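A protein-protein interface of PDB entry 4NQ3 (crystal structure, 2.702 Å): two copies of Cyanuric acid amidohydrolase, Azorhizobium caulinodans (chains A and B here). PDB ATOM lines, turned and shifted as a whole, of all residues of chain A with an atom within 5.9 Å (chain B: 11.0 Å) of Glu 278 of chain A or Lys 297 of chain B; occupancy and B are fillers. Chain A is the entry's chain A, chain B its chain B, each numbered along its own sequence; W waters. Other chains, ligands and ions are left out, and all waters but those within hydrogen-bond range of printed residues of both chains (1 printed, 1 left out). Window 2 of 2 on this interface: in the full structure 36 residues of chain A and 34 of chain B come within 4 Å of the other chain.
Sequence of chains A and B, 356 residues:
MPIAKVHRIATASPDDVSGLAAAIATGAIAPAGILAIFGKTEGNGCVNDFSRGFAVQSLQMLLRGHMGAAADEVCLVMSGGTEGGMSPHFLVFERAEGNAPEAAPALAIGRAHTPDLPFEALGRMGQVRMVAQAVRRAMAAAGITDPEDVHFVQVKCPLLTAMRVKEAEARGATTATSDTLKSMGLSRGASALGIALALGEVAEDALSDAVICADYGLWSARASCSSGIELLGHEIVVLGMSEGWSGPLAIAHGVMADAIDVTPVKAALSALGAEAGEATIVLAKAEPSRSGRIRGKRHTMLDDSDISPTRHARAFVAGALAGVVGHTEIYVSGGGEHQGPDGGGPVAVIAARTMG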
ATOM      1  N   ARG A   8     -28.048  27.030   1.739  1.00  0.00           N
ATOM      2  CA  ARG A   8     -26.950  27.670   2.469  1.00  0.00           C
ATOM      3  C   ARG A   8     -25.593  27.397   1.785  1.00  0.00           C
ATOM      4  O   ARG A   8     -25.143  26.265   1.683  1.00  0.00           O
ATOM      5  CB  ARG A   8     -26.921  27.209   3.917  1.00  0.00           C
ATOM      6  CG  ARG A   8     -26.272  28.199   4.850  1.00  0.00           C
ATOM      7  CD  ARG A   8     -26.534  27.852   6.342  1.00  0.00           C
ATOM      8  NE  ARG A   8     -25.910  26.575   6.670  1.00  0.00           N
ATOM      9  CZ  ARG A   8     -26.305  25.723   7.611  1.00  0.00           C
ATOM     10  NH1 ARG A   8     -27.349  25.965   8.396  1.00  0.00           N
ATOM     11  NH2 ARG A   8     -25.619  24.604   7.764  1.00  0.00           N
ATOM     12  N   GLY A  85     -16.599  32.785  16.146  1.00  0.00           N
ATOM     13  CA  GLY A  85     -16.376  31.708  15.206  1.00  0.00           C
ATOM     14  C   GLY A  85     -17.382  31.723  14.077  1.00  0.00           C
ATOM     15  O   GLY A  85     -17.375  30.837  13.233  1.00  0.00           O
ATOM     16  N   SER A  87     -19.429  31.835  10.863  1.00  0.00           N
ATOM     17  CA  SER A  87     -18.898  31.445   9.555  1.00  0.00           C
ATOM     18  C   SER A  87     -19.582  32.142   8.362  1.00  0.00           C
ATOM     19  O   SER A  87     -20.785  31.995   8.143  1.00  0.00           O
ATOM     20  CB  SER A  87     -19.021  29.929   9.419  1.00  0.00           C
ATOM     21  OG  SER A  87     -18.609  29.478   8.155  1.00  0.00           O
ATOM     22  N   ALA A 276     -31.505  19.897  16.515  1.00  0.00           N
ATOM     23  CA  ALA A 276     -30.319  20.644  16.126  1.00  0.00           C
ATOM     24  C   ALA A 276     -29.361  19.781  15.304  1.00  0.00           C
ATOM     25  O   ALA A 276     -29.106  18.613  15.626  1.00  0.00           O
ATOM     26  CB  ALA A 276     -29.616  21.205  17.363  1.00  0.00           C
ATOM     27  N   GLY A 277     -28.841  20.364  14.232  1.00  0.00           N
ATOM     28  CA  GLY A 277     -27.902  19.673  13.375  1.00  0.00           C
ATOM     29  C   GLY A 277     -27.330  20.641  12.364  1.00  0.00           C
ATOM     30  O   GLY A 277     -27.776  21.791  12.280  1.00  0.00           O
ATOM     31  N   GLU A 278     -26.343  20.177  11.598  1.00  0.00           N
ATOM     32  CA  GLU A 278     -25.686  21.013  10.609  1.00  0.00           C
ATOM     33  C   GLU A 278     -26.736  21.665   9.722  1.00  0.00           C
ATOM     34  O   GLU A 278     -26.596  22.812   9.324  1.00  0.00           O
ATOM     35  CB  GLU A 278     -24.689  20.186   9.782  1.00  0.00           C
ATOM     36  CG  GLU A 278     -23.635  21.002   9.018  1.00  0.00           C
ATOM     37  CD  GLU A 278     -24.035  21.323   7.583  1.00  0.00           C
ATOM     38  OE1 GLU A 278     -25.070  20.801   7.110  1.00  0.00           O
ATOM     39  OE2 GLU A 278     -23.316  22.109   6.929  1.00  0.00           O
ATOM     40  N   ALA A 279     -27.837  20.968   9.500  1.00  0.00           N
ATOM     41  CA  ALA A 279     -28.859  21.449   8.577  1.00  0.00           C
ATOM     42  C   ALA A 279     -29.745  22.556   9.143  1.00  0.00           C
ATOM     43  O   ALA A 279     -30.406  23.255   8.384  1.00  0.00           O
ATOM     44  CB  ALA A 279     -29.715  20.298   8.117  1.00  0.00           C
ATOM     45  N   THR A 280     -29.795  22.712  10.461  1.00  0.00           N
ATOM     46  CA  THR A 280     -30.641  23.763  11.040  1.00  0.00           C
ATOM     47  C   THR A 280     -30.223  25.154  10.528  1.00  0.00           C
ATOM     48  O   THR A 280     -29.040  25.497  10.505  1.00  0.00           O
ATOM     49  CB  THR A 280     -30.571  23.775  12.576  1.00  0.00           C
ATOM     50  OG1 THR A 280     -30.710  22.442  13.087  1.00  0.00           O
ATOM     51  CG2 THR A 280     -31.658  24.664  13.141  1.00  0.00           C
ATOM     52  N   ILE A 281     -31.191  25.939  10.083  1.00  0.00           N
ATOM     53  CA  ILE A 281     -30.926  27.303   9.665  1.00  0.00           C
ATOM     54  C   ILE A 281     -31.365  28.263  10.762  1.00  0.00           C
ATOM     55  O   ILE A 281     -32.524  28.207  11.197  1.00  0.00           O
ATOM     56  CB  ILE A 281     -31.686  27.632   8.391  1.00  0.00           C
ATOM     57  CG1 ILE A 281     -31.166  26.795   7.234  1.00  0.00           C
ATOM     58  CG2 ILE A 281     -31.619  29.129   8.099  1.00  0.00           C
ATOM     59  CD1 ILE A 281     -31.955  27.015   6.000  1.00  0.00           C
ATOM     60  N   VAL A 325     -26.950  24.764  18.624  1.00  0.00           N
ATOM     61  CA  VAL A 325     -27.335  24.196  17.353  1.00  0.00           C
ATOM     62  C   VAL A 325     -26.167  23.389  16.765  1.00  0.00           C
ATOM     63  O   VAL A 325     -26.340  22.644  15.811  1.00  0.00           O
ATOM     64  CB  VAL A 325     -27.829  25.318  16.399  1.00  0.00           C
ATOM     65  CG1 VAL A 325     -26.686  26.205  15.992  1.00  0.00           C
ATOM     66  CG2 VAL A 325     -28.506  24.744  15.188  1.00  0.00           C
ATOM     67  N   HIS A 327     -23.243  24.138  15.176  1.00  0.00           N
ATOM     68  CA  HIS A 327     -22.405  24.602  14.073  1.00  0.00           C
ATOM     69  C   HIS A 327     -22.350  26.110  14.025  1.00  0.00           C
ATOM     70  O   HIS A 327     -23.050  26.783  14.772  1.00  0.00           O
ATOM     71  CB  HIS A 327     -22.902  24.060  12.746  1.00  0.00           C
ATOM     72  CG  HIS A 327     -24.206  24.636  12.301  1.00  0.00           C
ATOM     73  ND1 HIS A 327     -24.291  25.661  11.383  1.00  0.00           N
ATOM     74  CD2 HIS A 327     -25.482  24.304  12.618  1.00  0.00           C
ATOM     75  CE1 HIS A 327     -25.565  25.944  11.161  1.00  0.00           C
ATOM     76  NE2 HIS A 327     -26.307  25.134  11.898  1.00  0.00           N
ATOM     77  N   THR A 328     -21.493  26.643  13.165  1.00  0.00           N
ATOM     78  CA  THR A 328     -21.228  28.071  13.192  1.00  0.00           C
ATOM     79  C   THR A 328     -21.703  28.797  11.953  1.00  0.00           C
ATOM     80  O   THR A 328     -21.465  29.990  11.809  1.00  0.00           O
ATOM     81  CB  THR A 328     -19.757  28.336  13.366  1.00  0.00           C
ATOM     82  OG1 THR A 328     -19.063  27.713  12.286  1.00  0.00           O
ATOM     83  CG2 THR A 328     -19.283  27.767  14.700  1.00  0.00           C
ATOM     84  N   GLU A 329     -22.374  28.090  11.054  1.00  0.00           N
ATOM     85  CA  GLU A 329     -22.878  28.733   9.844  1.00  0.00           C
ATOM     86  C   GLU A 329     -24.269  29.306  10.136  1.00  0.00           C
ATOM     87  O   GLU A 329     -25.256  28.861   9.575  1.00  0.00           O
ATOM     88  CB  GLU A 329     -22.931  27.746   8.670  1.00  0.00           C
ATOM     89  CG  GLU A 329     -22.425  28.268   7.325  1.00  0.00           C
ATOM     90  CD  GLU A 329     -22.220  27.137   6.315  1.00  0.00           C
ATOM     91  OE1 GLU A 329     -23.191  26.388   6.074  1.00  0.00           O
ATOM     92  OE2 GLU A 329     -21.092  26.967   5.784  1.00  0.00           O
ATOM     93  N   ASP B 258     -13.729  21.799  20.819  1.00  0.00           N
ATOM     94  CA  ASP B 258     -13.631  23.005  20.016  1.00  0.00           C
ATOM     95  C   ASP B 258     -14.378  24.141  20.707  1.00  0.00           C
ATOM     96  O   ASP B 258     -14.809  23.986  21.847  1.00  0.00           O
ATOM     97  CB  ASP B 258     -14.169  22.763  18.604  1.00  0.00           C
ATOM     98  CG  ASP B 258     -15.566  22.145  18.599  1.00  0.00           C
ATOM     99  OD1 ASP B 258     -16.349  22.397  19.543  1.00  0.00           O
ATOM    100  OD2 ASP B 258     -15.895  21.424  17.630  1.00  0.00           O
ATOM    101  N   ALA B 259     -14.529  25.273  20.022  1.00  0.00           N
ATOM    102  CA  ALA B 259     -15.030  26.488  20.668  1.00  0.00           C
ATOM    103  C   ALA B 259     -16.505  26.415  21.084  1.00  0.00           C
ATOM    104  O   ALA B 259     -16.941  27.216  21.903  1.00  0.00           O
ATOM    105  CB  ALA B 259     -14.801  27.704  19.760  1.00  0.00           C
ATOM    106  N   ILE B 260     -17.268  25.463  20.549  1.00  0.00           N
ATOM    107  CA  ILE B 260     -18.692  25.365  20.877  1.00  0.00           C
ATOM    108  C   ILE B 260     -19.048  24.045  21.518  1.00  0.00           C
ATOM    109  O   ILE B 260     -20.215  23.651  21.525  1.00  0.00           O
ATOM    110  CB  ILE B 260     -19.593  25.524  19.636  1.00  0.00           C
ATOM    111  CG1 ILE B 260     -19.245  24.465  18.595  1.00  0.00           C
ATOM    112  CG2 ILE B 260     -19.467  26.905  19.067  1.00  0.00           C
ATOM    113  CD1 ILE B 260     -20.072  24.542  17.342  1.00  0.00           C
ATOM    114  N   PRO B 288      -8.720  30.235  19.229  1.00  0.00           N
ATOM    115  CA  PRO B 288      -9.085  30.098  17.813  1.00  0.00           C
ATOM    116  C   PRO B 288      -8.375  28.898  17.215  1.00  0.00           C
ATOM    117  O   PRO B 288      -7.176  28.744  17.460  1.00  0.00           O
ATOM    118  CB  PRO B 288      -8.585  31.398  17.184  1.00  0.00           C
ATOM    119  CG  PRO B 288      -7.478  31.852  18.088  1.00  0.00           C
ATOM    120  CD  PRO B 288      -7.864  31.404  19.482  1.00  0.00           C
ATOM    121  N   SER B 289      -9.091  28.050  16.484  1.00  0.00           N
ATOM    122  CA  SER B 289      -8.489  26.830  15.953  1.00  0.00           C
ATOM    123  C   SER B 289      -7.614  27.187  14.777  1.00  0.00           C
ATOM    124  O   SER B 289      -8.009  27.974  13.921  1.00  0.00           O
ATOM    125  CB  SER B 289      -9.548  25.813  15.549  1.00  0.00           C
ATOM    126  OG  SER B 289     -10.377  26.352  14.547  1.00  0.00           O
ATOM    127  N   ARG B 290      -6.415  26.619  14.751  1.00  0.00           N
ATOM    128  CA  ARG B 290      -5.417  27.010  13.773  1.00  0.00           C
ATOM    129  C   ARG B 290      -5.712  26.414  12.426  1.00  0.00           C
ATOM    130  O   ARG B 290      -5.051  26.742  11.440  1.00  0.00           O
ATOM    131  CB  ARG B 290      -4.021  26.621  14.237  1.00  0.00           C
ATOM    132  CG  ARG B 290      -3.538  27.511  15.357  1.00  0.00           C
ATOM    133  CD  ARG B 290      -2.157  27.130  15.887  1.00  0.00           C
ATOM    134  NE  ARG B 290      -1.808  28.050  16.959  1.00  0.00           N
ATOM    135  CZ  ARG B 290      -2.098  27.857  18.244  1.00  0.00           C
ATOM    136  NH1 ARG B 290      -2.699  26.733  18.647  1.00  0.00           N
ATOM    137  NH2 ARG B 290      -1.753  28.790  19.134  1.00  0.00           N
ATOM    138  N   SER B 291      -6.701  25.531  12.383  1.00  0.00           N
ATOM    139  CA  SER B 291      -7.169  24.999  11.114  1.00  0.00           C
ATOM    140  C   SER B 291      -7.926  26.041  10.320  1.00  0.00           C
ATOM    141  O   SER B 291      -8.088  25.918   9.111  1.00  0.00           O
ATOM    142  CB  SER B 291      -8.065  23.796  11.348  1.00  0.00           C
ATOM    143  OG  SER B 291      -9.186  24.133  12.148  1.00  0.00           O
ATOM    144  N   GLY B 292      -8.386  27.085  11.000  1.00  0.00           N
ATOM    145  CA  GLY B 292      -9.226  28.073  10.354  1.00  0.00           C
ATOM    146  C   GLY B 292     -10.658  27.575  10.214  1.00  0.00           C
ATOM    147  O   GLY B 292     -11.466  28.172   9.483  1.00  0.00           O
ATOM    148  N   ARG B 293     -10.967  26.451  10.863  1.00  0.00           N
ATOM    149  CA  ARG B 293     -12.315  25.907  10.790  1.00  0.00           C
ATOM    150  C   ARG B 293     -12.825  25.476  12.145  1.00  0.00           C
ATOM    151  O   ARG B 293     -12.050  25.093  13.002  1.00  0.00           O
ATOM    152  CB  ARG B 293     -12.368  24.727   9.816  1.00  0.00           C
ATOM    153  CG  ARG B 293     -11.665  24.986   8.491  1.00  0.00           C
ATOM    154  CD  ARG B 293     -11.963  23.930   7.424  1.00  0.00           C
ATOM    155  NE  ARG B 293     -11.463  24.350   6.106  1.00  0.00           N
ATOM    156  CZ  ARG B 293     -12.200  24.905   5.138  1.00  0.00           C
ATOM    157  NH1 ARG B 293     -13.500  25.133   5.303  1.00  0.00           N
ATOM    158  NH2 ARG B 293     -11.629  25.250   3.994  1.00  0.00           N
ATOM    159  N   ILE B 294     -14.136  25.554  12.336  1.00  0.00           N
ATOM    160  CA  ILE B 294     -14.813  24.863  13.435  1.00  0.00           C
ATOM    161  C   ILE B 294     -15.817  23.881  12.842  1.00  0.00           C
ATOM    162  O   ILE B 294     -16.739  24.289  12.133  1.00  0.00           O
ATOM    163  CB  ILE B 294     -15.541  25.809  14.360  1.00  0.00           C
ATOM    164  CG1 ILE B 294     -14.561  26.813  14.961  1.00  0.00           C
ATOM    165  CG2 ILE B 294     -16.251  25.028  15.444  1.00  0.00           C
ATOM    166  CD1 ILE B 294     -15.241  27.810  15.902  1.00  0.00           C
ATOM    167  N   ARG B 295     -15.609  22.591  13.102  1.00  0.00           N
ATOM    168  CA  ARG B 295     -16.468  21.517  12.593  1.00  0.00           C
ATOM    169  C   ARG B 295     -16.701  21.657  11.099  1.00  0.00           C
ATOM    170  O   ARG B 295     -17.841  21.628  10.630  1.00  0.00           O
ATOM    171  CB  ARG B 295     -17.801  21.482  13.345  1.00  0.00           C
ATOM    172  CG  ARG B 295     -17.591  21.362  14.829  1.00  0.00           C
ATOM    173  CD  ARG B 295     -18.857  21.078  15.578  1.00  0.00           C
ATOM    174  NE  ARG B 295     -18.593  20.994  17.017  1.00  0.00           N
ATOM    175  CZ  ARG B 295     -19.539  20.857  17.942  1.00  0.00           C
ATOM    176  NH1 ARG B 295     -20.820  20.762  17.590  1.00  0.00           N
ATOM    177  NH2 ARG B 295     -19.205  20.810  19.222  1.00  0.00           N
ATOM    178  N   GLY B 296     -15.612  21.852  10.368  1.00  0.00           N
ATOM    179  CA  GLY B 296     -15.644  21.926   8.916  1.00  0.00           C
ATOM    180  C   GLY B 296     -15.864  23.316   8.354  1.00  0.00           C
ATOM    181  O   GLY B 296     -15.508  23.579   7.209  1.00  0.00           O
ATOM    182  N   LYS B 297     -16.414  24.213   9.172  1.00  0.00           N
ATOM    183  CA  LYS B 297     -16.826  25.549   8.727  1.00  0.00           C
ATOM    184  C   LYS B 297     -15.741  26.595   8.979  1.00  0.00           C
ATOM    185  O   LYS B 297     -15.173  26.673  10.084  1.00  0.00           O
ATOM    186  CB  LYS B 297     -18.116  25.968   9.430  1.00  0.00           C
ATOM    187  CG  LYS B 297     -19.258  25.005   9.257  1.00  0.00           C
ATOM    188  CD  LYS B 297     -19.663  24.990   7.799  1.00  0.00           C
ATOM    189  CE  LYS B 297     -20.775  23.997   7.543  1.00  0.00           C
ATOM    190  NZ  LYS B 297     -21.996  24.331   8.329  1.00  0.00           N
ATOM    191  N   ARG B 298     -15.444  27.399   7.962  1.00  0.00           N
ATOM    192  CA  ARG B 298     -14.354  28.351   8.122  1.00  0.00           C
ATOM    193  C   ARG B 298     -14.745  29.453   9.106  1.00  0.00           C
ATOM    194  O   ARG B 298     -15.918  29.828   9.191  1.00  0.00           O
ATOM    195  CB  ARG B 298     -13.957  28.933   6.775  1.00  0.00           C
ATOM    196  CG  ARG B 298     -14.170  30.411   6.636  1.00  0.00           C
ATOM    197  CD  ARG B 298     -13.456  30.939   5.388  1.00  0.00           C
ATOM    198  NE  ARG B 298     -14.297  31.930   4.743  1.00  0.00           N
ATOM    199  CZ  ARG B 298     -14.111  33.245   4.818  1.00  0.00           C
ATOM    200  NH1 ARG B 298     -13.069  33.739   5.484  1.00  0.00           N
ATOM    201  NH2 ARG B 298     -14.966  34.064   4.205  1.00  0.00           N
ATOM    202  N   HIS B 299     -13.766  29.943   9.864  1.00  0.00           N
ATOM    203  CA  HIS B 299     -13.966  31.082  10.762  1.00  0.00           C
ATOM    204  C   HIS B 299     -12.969  32.147  10.382  1.00  0.00           C
ATOM    205  O   HIS B 299     -12.092  31.884   9.574  1.00  0.00           O
ATOM    206  CB  HIS B 299     -13.804  30.693  12.222  1.00  0.00           C
ATOM    207  CG  HIS B 299     -12.414  30.287  12.592  1.00  0.00           C
ATOM    208  ND1 HIS B 299     -11.349  31.159  12.556  1.00  0.00           N
ATOM    209  CD2 HIS B 299     -11.917  29.101  13.022  1.00  0.00           C
ATOM    210  CE1 HIS B 299     -10.253  30.527  12.939  1.00  0.00           C
ATOM    211  NE2 HIS B 299     -10.569  29.275  13.224  1.00  0.00           N
ATOM    212  N   THR B 300     -13.102  33.350  10.932  1.00  0.00           N
ATOM    213  CA  THR B 300     -12.277  34.449  10.432  1.00  0.00           C
ATOM    214  C   THR B 300     -11.279  35.028  11.422  1.00  0.00           C
ATOM    215  O   THR B 300     -10.652  36.040  11.117  1.00  0.00           O
ATOM    216  CB  THR B 300     -13.152  35.608   9.929  1.00  0.00           C
ATOM    217  OG1 THR B 300     -13.794  36.240  11.034  1.00  0.00           O
ATOM    218  CG2 THR B 300     -14.200  35.085   8.981  1.00  0.00           C
ATOM    219  N   MET B 301     -11.120  34.373  12.574  1.00  0.00           N
ATOM    220  CA  MET B 301     -10.373  34.915  13.719  1.00  0.00           C
ATOM    221  C   MET B 301      -8.882  35.119  13.448  1.00  0.00           C
ATOM    222  O   MET B 301      -8.281  36.059  13.963  1.00  0.00           O
ATOM    223  CB  MET B 301     -10.552  34.002  14.950  1.00  0.00           C
ATOM    224  CG  MET B 301     -11.943  34.076  15.575  1.00  0.00           C
ATOM    225  SD  MET B 301     -12.354  32.744  16.940  1.00  0.00           S
ATOM    226  CE  MET B 301     -11.978  31.125  15.934  1.00  0.00           C
ATOM    227  N   LEU B 302      -8.295  34.253  12.628  1.00  0.00           N
ATOM    228  CA  LEU B 302      -6.864  34.302  12.356  1.00  0.00           C
ATOM    229  C   LEU B 302      -6.501  35.266  11.240  1.00  0.00           C
ATOM    230  O   LEU B 302      -5.328  35.454  10.936  1.00  0.00           O
ATOM    231  CB  LEU B 302      -6.352  32.907  12.012  1.00  0.00           C
ATOM    232  CG  LEU B 302      -6.470  31.959  13.198  1.00  0.00           C
ATOM    233  CD1 LEU B 302      -5.921  30.623  12.845  1.00  0.00           C
ATOM    234  CD2 LEU B 302      -5.724  32.527  14.366  1.00  0.00           C
ATOM    235  N   ASP B 303      -7.506  35.851  10.605  1.00  0.00           N
ATOM    236  CA  ASP B 303      -7.289  36.682   9.422  1.00  0.00           C
ATOM    237  C   ASP B 303      -7.733  38.120   9.686  1.00  0.00           C
ATOM    238  O   ASP B 303      -7.776  38.937   8.771  1.00  0.00           O
ATOM    239  CB  ASP B 303      -8.038  36.099   8.207  1.00  0.00           C
ATOM    240  CG  ASP B 303      -7.482  34.733   7.749  1.00  0.00           C
ATOM    241  OD1 ASP B 303      -6.244  34.563   7.745  1.00  0.00           O
ATOM    242  OD2 ASP B 303      -8.271  33.823   7.390  1.00  0.00           O
ATOM    243  N   PHE B 316     -16.615  34.566  21.934  1.00  0.00           N
ATOM    244  CA  PHE B 316     -17.390  33.461  21.390  1.00  0.00           C
ATOM    245  C   PHE B 316     -17.643  32.346  22.400  1.00  0.00           C
ATOM    246  O   PHE B 316     -18.792  31.953  22.572  1.00  0.00           O
ATOM    247  CB  PHE B 316     -16.697  32.901  20.145  1.00  0.00           C
ATOM    248  CG  PHE B 316     -17.588  32.069  19.269  1.00  0.00           C
ATOM    249  CD1 PHE B 316     -18.664  32.638  18.615  1.00  0.00           C
ATOM    250  CD2 PHE B 316     -17.324  30.727  19.057  1.00  0.00           C
ATOM    251  CE1 PHE B 316     -19.484  31.876  17.786  1.00  0.00           C
ATOM    252  CE2 PHE B 316     -18.138  29.957  18.221  1.00  0.00           C
ATOM    253  CZ  PHE B 316     -19.221  30.535  17.594  1.00  0.00           C
ATOM    254  N   GLY B 343      -7.667  24.396  19.126  1.00  0.00           N
ATOM    255  CA  GLY B 343      -9.007  24.895  18.867  1.00  0.00           C
ATOM    256  C   GLY B 343      -9.887  24.719  20.086  1.00  0.00           C
ATOM    257  O   GLY B 343     -10.978  25.286  20.154  1.00  0.00           O
HETATM  258  O   HOH W   1     -19.546  24.482  12.646  1.00  0.00           O
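A ring nitrogen (NE2) of His 327 of chain A sits at hydrogen-bond distance from the backbone carbonyl oxygen (O) of Glu 278 of chain A (3.5 Å).
NH2 of Arg 8 of chain A is in salt-bridge range of OE2 of Glu 278 of chain A (3.5 Å).
The backbone carbonyl oxygen (O) of Thr 328 of chain A sits at hydrogen-bond distance from the backbone NH (N) of Ser 87 of chain A.
The guanidinium group (NH1) of Arg 8 of chain A lies within hydrogen-bond range of the backbone carbonyl oxygen (O) of Thr 280 of chain A (2.7 Å).
A ring nitrogen (ND1) of His 327 of chain A sits at hydrogen-bond distance from the backbone NH of Glu 329 of chain A, at 3.1 Å.
NE2 of His 327 of chain A lies within hydrogen-bond range of O of Thr 280 of chain A (3.1 Å).
Of the 13 printed residues of chain A, 7 touch a printed residue of chain B.
Hydrophobic or aromatic side chains of chain B that line the printed part of chain A: Ile 260, His 299 and Phe 316.
Among the printed residues, Asp or Glu carboxylates within 4 Å of a Lys or Arg side-chain nitrogen of the other chain: Glu 278 of chain A with Lys 297 of chain B and Glu 329 of chain A with Lys 297 of chain B.
Of chain B, only Lys 297 (3.8 Å) and Arg 298 (2.9 Å) come within 4 Å of Ser 87 of chain A.
Glu 278 of chain A touches one residue of chain B.
No residue of chain B comes within 4 Å of Thr 280 of chain A.
Printed residues of chain B within 4 Å of Thr 328 of chain A: Lys 297.
Of chain B, only Lys 297 comes within 4 Å of Glu 329 of chain A.
Lys 297 of chain B touches just these residues of chain A: Arg 8, Ser 87, Glu 278, Thr 328 and Glu 329.
Of the printed residues of chain A, His 299 of chain B touches Gly 85 (3.7 Å).
The nearest residue of chain B that does not touch Glu 278 of chain A is Arg 295 of chain B (6.0 Å).
The nearest residue of chain A that does not touch Lys 297 of chain B is His 327 of chain A (4.05 Å).
The nearest printed residue of chain B that does not touch Gly 85 of chain A is Ile 294 of chain B (4.1 Å).
Water W1 lies within hydrogen-bond range of O of Ile 294 of chain B and N of Thr 328 of chain A.
No position is printed for both chains.
Of the 9 pairs that touch across the chains among the printed residues, none has its exchanged pair printed and touching as well.
The side-chain carboxylate (OE1) of Glu 329 of chain A lies within salt-bridge range of the side-chain amino group (NZ) of Lys 297 of chain B (3.3 Å).
The backbone carbonyl oxygen of Arg 298 of chain B is in hydrogen-bond range of the side-chain hydroxyl of Ser 87 of chain A (2.9 Å).
NZ of Lys 297 of chain B lies within salt-bridge range of OE2 of Glu 278 of chain A, 2.9 Å away.
NH2 of Arg 8 of chain A touches NZ of Lys 297 of chain B, at 3.7 Å.
O of Gly 85 of chain A touches CB of His 299 of chain B, 3.7 Å away.
Gly 85 of chain A touches Phe 316 of chain B.
CB of Lys 297 of chain B touches OG of Ser 87 of chain A (3.8 Å).
N of His 327 of chain A touches CD1 of Ile 260 of chain B (3.9 Å).
Thr 328 of chain A touches Lys 297 of chain B (OG1 to CB, 3.5 Å).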
